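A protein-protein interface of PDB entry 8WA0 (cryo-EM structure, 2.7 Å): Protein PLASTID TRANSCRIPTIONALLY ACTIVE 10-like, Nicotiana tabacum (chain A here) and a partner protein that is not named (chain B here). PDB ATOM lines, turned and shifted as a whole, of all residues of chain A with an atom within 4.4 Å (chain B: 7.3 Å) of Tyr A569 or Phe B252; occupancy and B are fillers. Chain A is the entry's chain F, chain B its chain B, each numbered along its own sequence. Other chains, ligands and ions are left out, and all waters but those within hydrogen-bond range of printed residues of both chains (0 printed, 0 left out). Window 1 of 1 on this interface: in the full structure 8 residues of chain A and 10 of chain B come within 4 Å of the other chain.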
ATOM      1  N   ASP A 563      33.048  -8.326  -8.207  1.00  0.00           N
ATOM      2  CA  ASP A 563      32.721  -7.478  -7.051  1.00  0.00           C
ATOM      3  C   ASP A 563      33.389  -7.882  -5.738  1.00  0.00           C
ATOM      4  O   ASP A 563      33.137  -7.281  -4.699  1.00  0.00           O
ATOM      5  CB  ASP A 563      31.202  -7.458  -6.842  1.00  0.00           C
ATOM      6  CG  ASP A 563      30.439  -7.098  -8.103  1.00  0.00           C
ATOM      7  OD1 ASP A 563      30.501  -7.865  -9.087  1.00  0.00           O
ATOM      8  OD2 ASP A 563      29.759  -6.052  -8.106  1.00  0.00           O
ATOM      9  N   TYR A 567      35.882  -3.883  -6.717  1.00  0.00           N
ATOM     10  CA  TYR A 567      36.244  -3.024  -7.823  1.00  0.00           C
ATOM     11  C   TYR A 567      34.979  -2.763  -8.595  1.00  0.00           C
ATOM     12  O   TYR A 567      34.733  -1.640  -9.031  1.00  0.00           O
ATOM     13  CB  TYR A 567      37.339  -3.647  -8.692  1.00  0.00           C
ATOM     14  CG  TYR A 567      38.733  -3.231  -8.313  1.00  0.00           C
ATOM     15  CD1 TYR A 567      39.363  -3.773  -7.207  1.00  0.00           C
ATOM     16  CD2 TYR A 567      39.423  -2.297  -9.067  1.00  0.00           C
ATOM     17  CE1 TYR A 567      40.644  -3.394  -6.856  1.00  0.00           C
ATOM     18  CE2 TYR A 567      40.704  -1.909  -8.727  1.00  0.00           C
ATOM     19  CZ  TYR A 567      41.310  -2.461  -7.619  1.00  0.00           C
ATOM     20  OH  TYR A 567      42.586  -2.080  -7.277  1.00  0.00           O
ATOM     21  N   ARG A 568      34.170  -3.791  -8.772  1.00  0.00           N
ATOM     22  CA  ARG A 568      32.893  -3.613  -9.431  1.00  0.00           C
ATOM     23  C   ARG A 568      31.880  -3.131  -8.430  1.00  0.00           C
ATOM     24  O   ARG A 568      32.079  -3.251  -7.228  1.00  0.00           O
ATOM     25  CB  ARG A 568      32.411  -4.912 -10.056  1.00  0.00           C
ATOM     26  N   TYR A 569      30.779  -2.598  -8.920  1.00  0.00           N
ATOM     27  CA  TYR A 569      29.793  -2.070  -8.013  1.00  0.00           C
ATOM     28  C   TYR A 569      28.598  -2.980  -7.923  1.00  0.00           C
ATOM     29  O   TYR A 569      27.936  -3.264  -8.919  1.00  0.00           O
ATOM     30  CB  TYR A 569      29.398  -0.627  -8.384  1.00  0.00           C
ATOM     31  CG  TYR A 569      28.661  -0.456  -9.699  1.00  0.00           C
ATOM     32  CD1 TYR A 569      29.329  -0.546 -10.913  1.00  0.00           C
ATOM     33  CD2 TYR A 569      27.299  -0.183  -9.721  1.00  0.00           C
ATOM     34  CE1 TYR A 569      28.658  -0.390 -12.110  1.00  0.00           C
ATOM     35  CE2 TYR A 569      26.622  -0.026 -10.913  1.00  0.00           C
ATOM     36  CZ  TYR A 569      27.305  -0.127 -12.103  1.00  0.00           C
ATOM     37  OH  TYR A 569      26.631   0.034 -13.291  1.00  0.00           O
ATOM     38  N   ASP A 570      28.209  -3.349  -6.707  1.00  0.00           N
ATOM     39  CA  ASP A 570      26.968  -4.108  -6.548  1.00  0.00           C
ATOM     40  C   ASP A 570      25.892  -3.037  -6.500  1.00  0.00           C
ATOM     41  O   ASP A 570      26.206  -1.853  -6.375  1.00  0.00           O
ATOM     42  CB  ASP A 570      26.978  -4.921  -5.259  1.00  0.00           C
ATOM     43  N   TYR A 571      24.625  -3.415  -6.578  1.00  0.00           N
ATOM     44  CA  TYR A 571      23.592  -2.385  -6.645  1.00  0.00           C
ATOM     45  C   TYR A 571      22.716  -2.259  -5.413  1.00  0.00           C
ATOM     46  O   TYR A 571      22.077  -3.223  -5.004  1.00  0.00           O
ATOM     47  CB  TYR A 571      22.708  -2.621  -7.872  1.00  0.00           C
ATOM     48  N   TRP A 572      22.680  -1.074  -4.815  1.00  0.00           N
ATOM     49  CA  TRP A 572      21.786  -0.846  -3.685  1.00  0.00           C
ATOM     50  C   TRP A 572      20.963   0.386  -4.005  1.00  0.00           C
ATOM     51  O   TRP A 572      21.526   1.464  -4.186  1.00  0.00           O
ATOM     52  CB  TRP A 572      22.588  -0.626  -2.406  1.00  0.00           C
ATOM     53  N   GLY A 573      19.640   0.254  -4.053  1.00  0.00           N
ATOM     54  CA  GLY A 573      18.789   1.374  -4.446  1.00  0.00           C
ATOM     55  C   GLY A 573      19.198   1.851  -5.821  1.00  0.00           C
ATOM     56  O   GLY A 573      19.146   3.047  -6.102  1.00  0.00           O
ATOM     57  N   GLU A 574      19.580   0.924  -6.696  1.00  0.00           N
ATOM     58  CA  GLU A 574      20.106   1.319  -8.002  1.00  0.00           C
ATOM     59  C   GLU A 574      19.380   0.828  -9.235  1.00  0.00           C
ATOM     60  O   GLU A 574      19.204  -0.374  -9.420  1.00  0.00           O
ATOM     61  CB  GLU A 574      21.532   0.804  -8.113  1.00  0.00           C
ATOM     62  N   MET B 187      27.654  -2.683   0.944  1.00  0.00           N
ATOM     63  CA  MET B 187      28.111  -3.046  -0.382  1.00  0.00           C
ATOM     64  C   MET B 187      28.370  -4.527  -0.443  1.00  0.00           C
ATOM     65  O   MET B 187      28.721  -5.066  -1.486  1.00  0.00           O
ATOM     66  CB  MET B 187      29.380  -2.277  -0.741  1.00  0.00           C
ATOM     67  N   PHE B 251      20.262   7.624  -2.861  1.00  0.00           N
ATOM     68  CA  PHE B 251      21.710   7.736  -2.816  1.00  0.00           C
ATOM     69  C   PHE B 251      22.323   7.409  -4.160  1.00  0.00           C
ATOM     70  O   PHE B 251      23.018   8.234  -4.743  1.00  0.00           O
ATOM     71  CB  PHE B 251      22.288   6.810  -1.753  1.00  0.00           C
ATOM     72  CG  PHE B 251      23.782   6.680  -1.814  1.00  0.00           C
ATOM     73  CD1 PHE B 251      24.596   7.734  -1.444  1.00  0.00           C
ATOM     74  CD2 PHE B 251      24.372   5.501  -2.239  1.00  0.00           C
ATOM     75  CE1 PHE B 251      25.970   7.621  -1.503  1.00  0.00           C
ATOM     76  CE2 PHE B 251      25.746   5.381  -2.301  1.00  0.00           C
ATOM     77  CZ  PHE B 251      26.547   6.443  -1.931  1.00  0.00           C
ATOM     78  N   PHE B 252      22.065   6.211  -4.664  1.00  0.00           N
ATOM     79  CA  PHE B 252      22.682   5.799  -5.916  1.00  0.00           C
ATOM     80  C   PHE B 252      22.249   6.682  -7.057  1.00  0.00           C
ATOM     81  O   PHE B 252      23.051   7.032  -7.919  1.00  0.00           O
ATOM     82  CB  PHE B 252      22.362   4.338  -6.247  1.00  0.00           C
ATOM     83  CG  PHE B 252      23.154   3.791  -7.404  1.00  0.00           C
ATOM     84  CD1 PHE B 252      22.687   3.904  -8.705  1.00  0.00           C
ATOM     85  CD2 PHE B 252      24.369   3.166  -7.188  1.00  0.00           C
ATOM     86  CE1 PHE B 252      23.419   3.411  -9.767  1.00  0.00           C
ATOM     87  CE2 PHE B 252      25.105   2.667  -8.246  1.00  0.00           C
ATOM     88  CZ  PHE B 252      24.629   2.789  -9.536  1.00  0.00           C
ATOM     89  N   GLN B 253      20.989   7.071  -7.069  1.00  0.00           N
ATOM     90  CA  GLN B 253      20.507   7.815  -8.213  1.00  0.00           C
ATOM     91  C   GLN B 253      21.253   9.118  -8.427  1.00  0.00           C
ATOM     92  O   GLN B 253      21.652   9.410  -9.552  1.00  0.00           O
ATOM     93  CB  GLN B 253      19.003   8.065  -8.057  1.00  0.00           C
ATOM     94  CG  GLN B 253      18.431   9.168  -8.932  1.00  0.00           C
ATOM     95  CD  GLN B 253      18.103  10.418  -8.140  1.00  0.00           C
ATOM     96  OE1 GLN B 253      17.850  10.353  -6.937  1.00  0.00           O
ATOM     97  NE2 GLN B 253      18.108  11.563  -8.810  1.00  0.00           N
ATOM     98  N   GLN B 254      21.467   9.876  -7.361  1.00  0.00           N
ATOM     99  CA  GLN B 254      22.104  11.181  -7.503  1.00  0.00           C
ATOM    100  C   GLN B 254      23.595  11.162  -7.248  1.00  0.00           C
ATOM    101  O   GLN B 254      24.388  11.354  -8.165  1.00  0.00           O
ATOM    102  CB  GLN B 254      21.430  12.183  -6.568  1.00  0.00           C
ATOM    103  N   ARG B 255      23.987  10.927  -6.008  1.00  0.00           N
ATOM    104  CA  ARG B 255      25.393  10.980  -5.665  1.00  0.00           C
ATOM    105  C   ARG B 255      26.251   9.948  -6.356  1.00  0.00           C
ATOM    106  O   ARG B 255      27.360  10.256  -6.777  1.00  0.00           O
ATOM    107  CB  ARG B 255      25.541  10.845  -4.159  1.00  0.00           C
ATOM    108  CG  ARG B 255      24.735  11.869  -3.381  1.00  0.00           C
ATOM    109  CD  ARG B 255      24.355  11.325  -2.018  1.00  0.00           C
ATOM    110  NE  ARG B 255      23.510  12.251  -1.274  1.00  0.00           N
ATOM    111  CZ  ARG B 255      22.916  11.952  -0.124  1.00  0.00           C
ATOM    112  NH1 ARG B 255      23.070  10.748   0.408  1.00  0.00           N
ATOM    113  NH2 ARG B 255      22.164  12.854   0.490  1.00  0.00           N
ATOM    114  N   CYS B 256      25.761   8.728  -6.493  1.00  0.00           N
ATOM    115  CA  CYS B 256      26.613   7.674  -7.043  1.00  0.00           C
ATOM    116  C   CYS B 256      27.056   7.846  -8.483  1.00  0.00           C
ATOM    117  O   CYS B 256      28.018   7.217  -8.904  1.00  0.00           O
ATOM    118  CB  CYS B 256      26.006   6.293  -6.829  1.00  0.00           C
ATOM    119  N   GLU B 257      26.374   8.679  -9.253  1.00  0.00           N
ATOM    120  CA  GLU B 257      26.854   8.923 -10.600  1.00  0.00           C
ATOM    121  C   GLU B 257      27.880  10.022 -10.600  1.00  0.00           C
ATOM    122  O   GLU B 257      27.646  11.102 -10.065  1.00  0.00           O
ATOM    123  CB  GLU B 257      25.706   9.294 -11.532  1.00  0.00           C
ATOM    124  N   ASN B 278      33.718   3.201 -16.869  1.00  0.00           N
ATOM    125  CA  ASN B 278      33.079   3.141 -15.556  1.00  0.00           C
ATOM    126  C   ASN B 278      32.821   4.556 -15.104  1.00  0.00           C
ATOM    127  O   ASN B 278      33.676   5.409 -15.254  1.00  0.00           O
ATOM    128  CB  ASN B 278      33.964   2.432 -14.538  1.00  0.00           C
ATOM    129  CG  ASN B 278      34.182   0.977 -14.864  1.00  0.00           C
ATOM    130  OD1 ASN B 278      33.742   0.099 -14.123  1.00  0.00           O
ATOM    131  ND2 ASN B 278      34.866   0.707 -15.968  1.00  0.00           N
ATOM    132  N   THR B 279      31.654   4.828 -14.548  1.00  0.00           N
ATOM    133  CA  THR B 279      31.314   6.181 -14.154  1.00  0.00           C
ATOM    134  C   THR B 279      30.487   6.117 -12.924  1.00  0.00           C
ATOM    135  O   THR B 279      29.449   6.763 -12.849  1.00  0.00           O
ATOM    136  CB  THR B 279      30.416   6.858 -15.192  1.00  0.00           C
ATOM    137  OG1 THR B 279      29.365   5.961 -15.568  1.00  0.00           O
ATOM    138  CG2 THR B 279      31.199   7.268 -16.433  1.00  0.00           C
ATOM    139  N   PHE B 280      30.920   5.357 -11.936  1.00  0.00           N
ATOM    140  CA  PHE B 280      30.068   5.161 -10.770  1.00  0.00           C
ATOM    141  C   PHE B 280      30.770   5.289  -9.442  1.00  0.00           C
ATOM    142  O   PHE B 280      31.985   5.212  -9.380  1.00  0.00           O
ATOM    143  CB  PHE B 280      29.388   3.800 -10.885  1.00  0.00           C
ATOM    144  CG  PHE B 280      28.448   3.695 -12.051  1.00  0.00           C
ATOM    145  CD1 PHE B 280      27.177   4.229 -11.979  1.00  0.00           C
ATOM    146  CD2 PHE B 280      28.849   3.090 -13.230  1.00  0.00           C
ATOM    147  CE1 PHE B 280      26.316   4.146 -13.054  1.00  0.00           C
ATOM    148  CE2 PHE B 280      27.995   3.003 -14.308  1.00  0.00           C
ATOM    149  CZ  PHE B 280      26.726   3.533 -14.220  1.00  0.00           C
ATOM    150  N   LEU B 281      30.022   5.493  -8.371  1.00  0.00           N
ATOM    151  CA  LEU B 281      30.656   5.510  -7.058  1.00  0.00           C
ATOM    152  C   LEU B 281      30.825   4.080  -6.600  1.00  0.00           C
ATOM    153  O   LEU B 281      30.159   3.639  -5.676  1.00  0.00           O
ATOM    154  CB  LEU B 281      29.825   6.276  -6.040  1.00  0.00           C
ATOM    155  CG  LEU B 281      30.551   6.820  -4.816  1.00  0.00           C
ATOM    156  CD1 LEU B 281      31.919   7.369  -5.188  1.00  0.00           C
ATOM    157  CD2 LEU B 281      29.698   7.891  -4.164  1.00  0.00           C
ATOM    158  N   LEU B 282      31.736   3.355  -7.234  1.00  0.00           N
ATOM    159  CA  LEU B 282      31.983   1.986  -6.869  1.00  0.00           C
ATOM    160  C   LEU B 282      32.548   2.023  -5.465  1.00  0.00           C
ATOM    161  O   LEU B 282      33.189   2.995  -5.073  1.00  0.00           O
ATOM    162  CB  LEU B 282      32.998   1.372  -7.821  1.00  0.00           C
ATOM    163  N   PRO B 283      32.308   0.979  -4.684  1.00  0.00           N
ATOM    164  CA  PRO B 283      32.762   1.038  -3.292  1.00  0.00           C
ATOM    165  C   PRO B 283      34.269   1.131  -2.934  1.00  0.00           C
ATOM    166  O   PRO B 283      34.535   1.656  -1.857  1.00  0.00           O
ATOM    167  CB  PRO B 283      32.041  -0.157  -2.639  1.00  0.00           C
ATOM    168  CG  PRO B 283      30.795  -0.290  -3.435  1.00  0.00           C
ATOM    169  CD  PRO B 283      31.205   0.018  -4.849  1.00  0.00           C
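Leu B282 touches Tyr A567.
Tyr A569 touches Phe B252.
Tyr A569 touches Phe B280.
Tyr A569 touches Leu B282.
CB of Phe B252 touches O of Trp A572 (3.6 Å).
Gly A573 touches Phe B252 (O to CB, 3.5 Å).
CD1 of Phe B252 touches CB of Glu A574, 3.4 Å away.
Of chain A, only Tyr A569 (3.7 Å), Trp A572 (3.6 Å), Gly A573 (3.5 Å) and Glu A574 (3.4 Å) come within 4 Å of Phe B252.
Printed residues of chain B within 4 Å of Trp A572: Phe B252.
Of the printed residues of chain B, Gly A573 touches Phe B252.
Of the printed residues of chain B, Tyr A567 touches Leu B282 (3.7 Å).
Arg A568 touches none of the printed residues of chain B.
Gln B254 touches none of the printed residues of chain A.
The nearest printed residue of chain A that does not touch Phe B252 is Asp A570 (5.0 Å).
The nearest printed residue of chain B that does not touch Tyr A567 is Asn B278 (5.5 Å).
Of the 9 printed residues of chain A, 5 touch a printed residue of chain B.
Printed residues of chain B that touch a printed residue of chain A: Phe B252, Phe B280 and Leu B282.
Hydrophobic or aromatic side chains of chain B within 4 Å of the printed part of chain A: Phe B252, Phe B280 and Leu B282.
Among the printed residues, 7 pairs touch across the chains.
Among the printed residues, no Asp or Glu carboxylate lies within 4 Å of a Lys or Arg side-chain nitrogen of the other chain.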
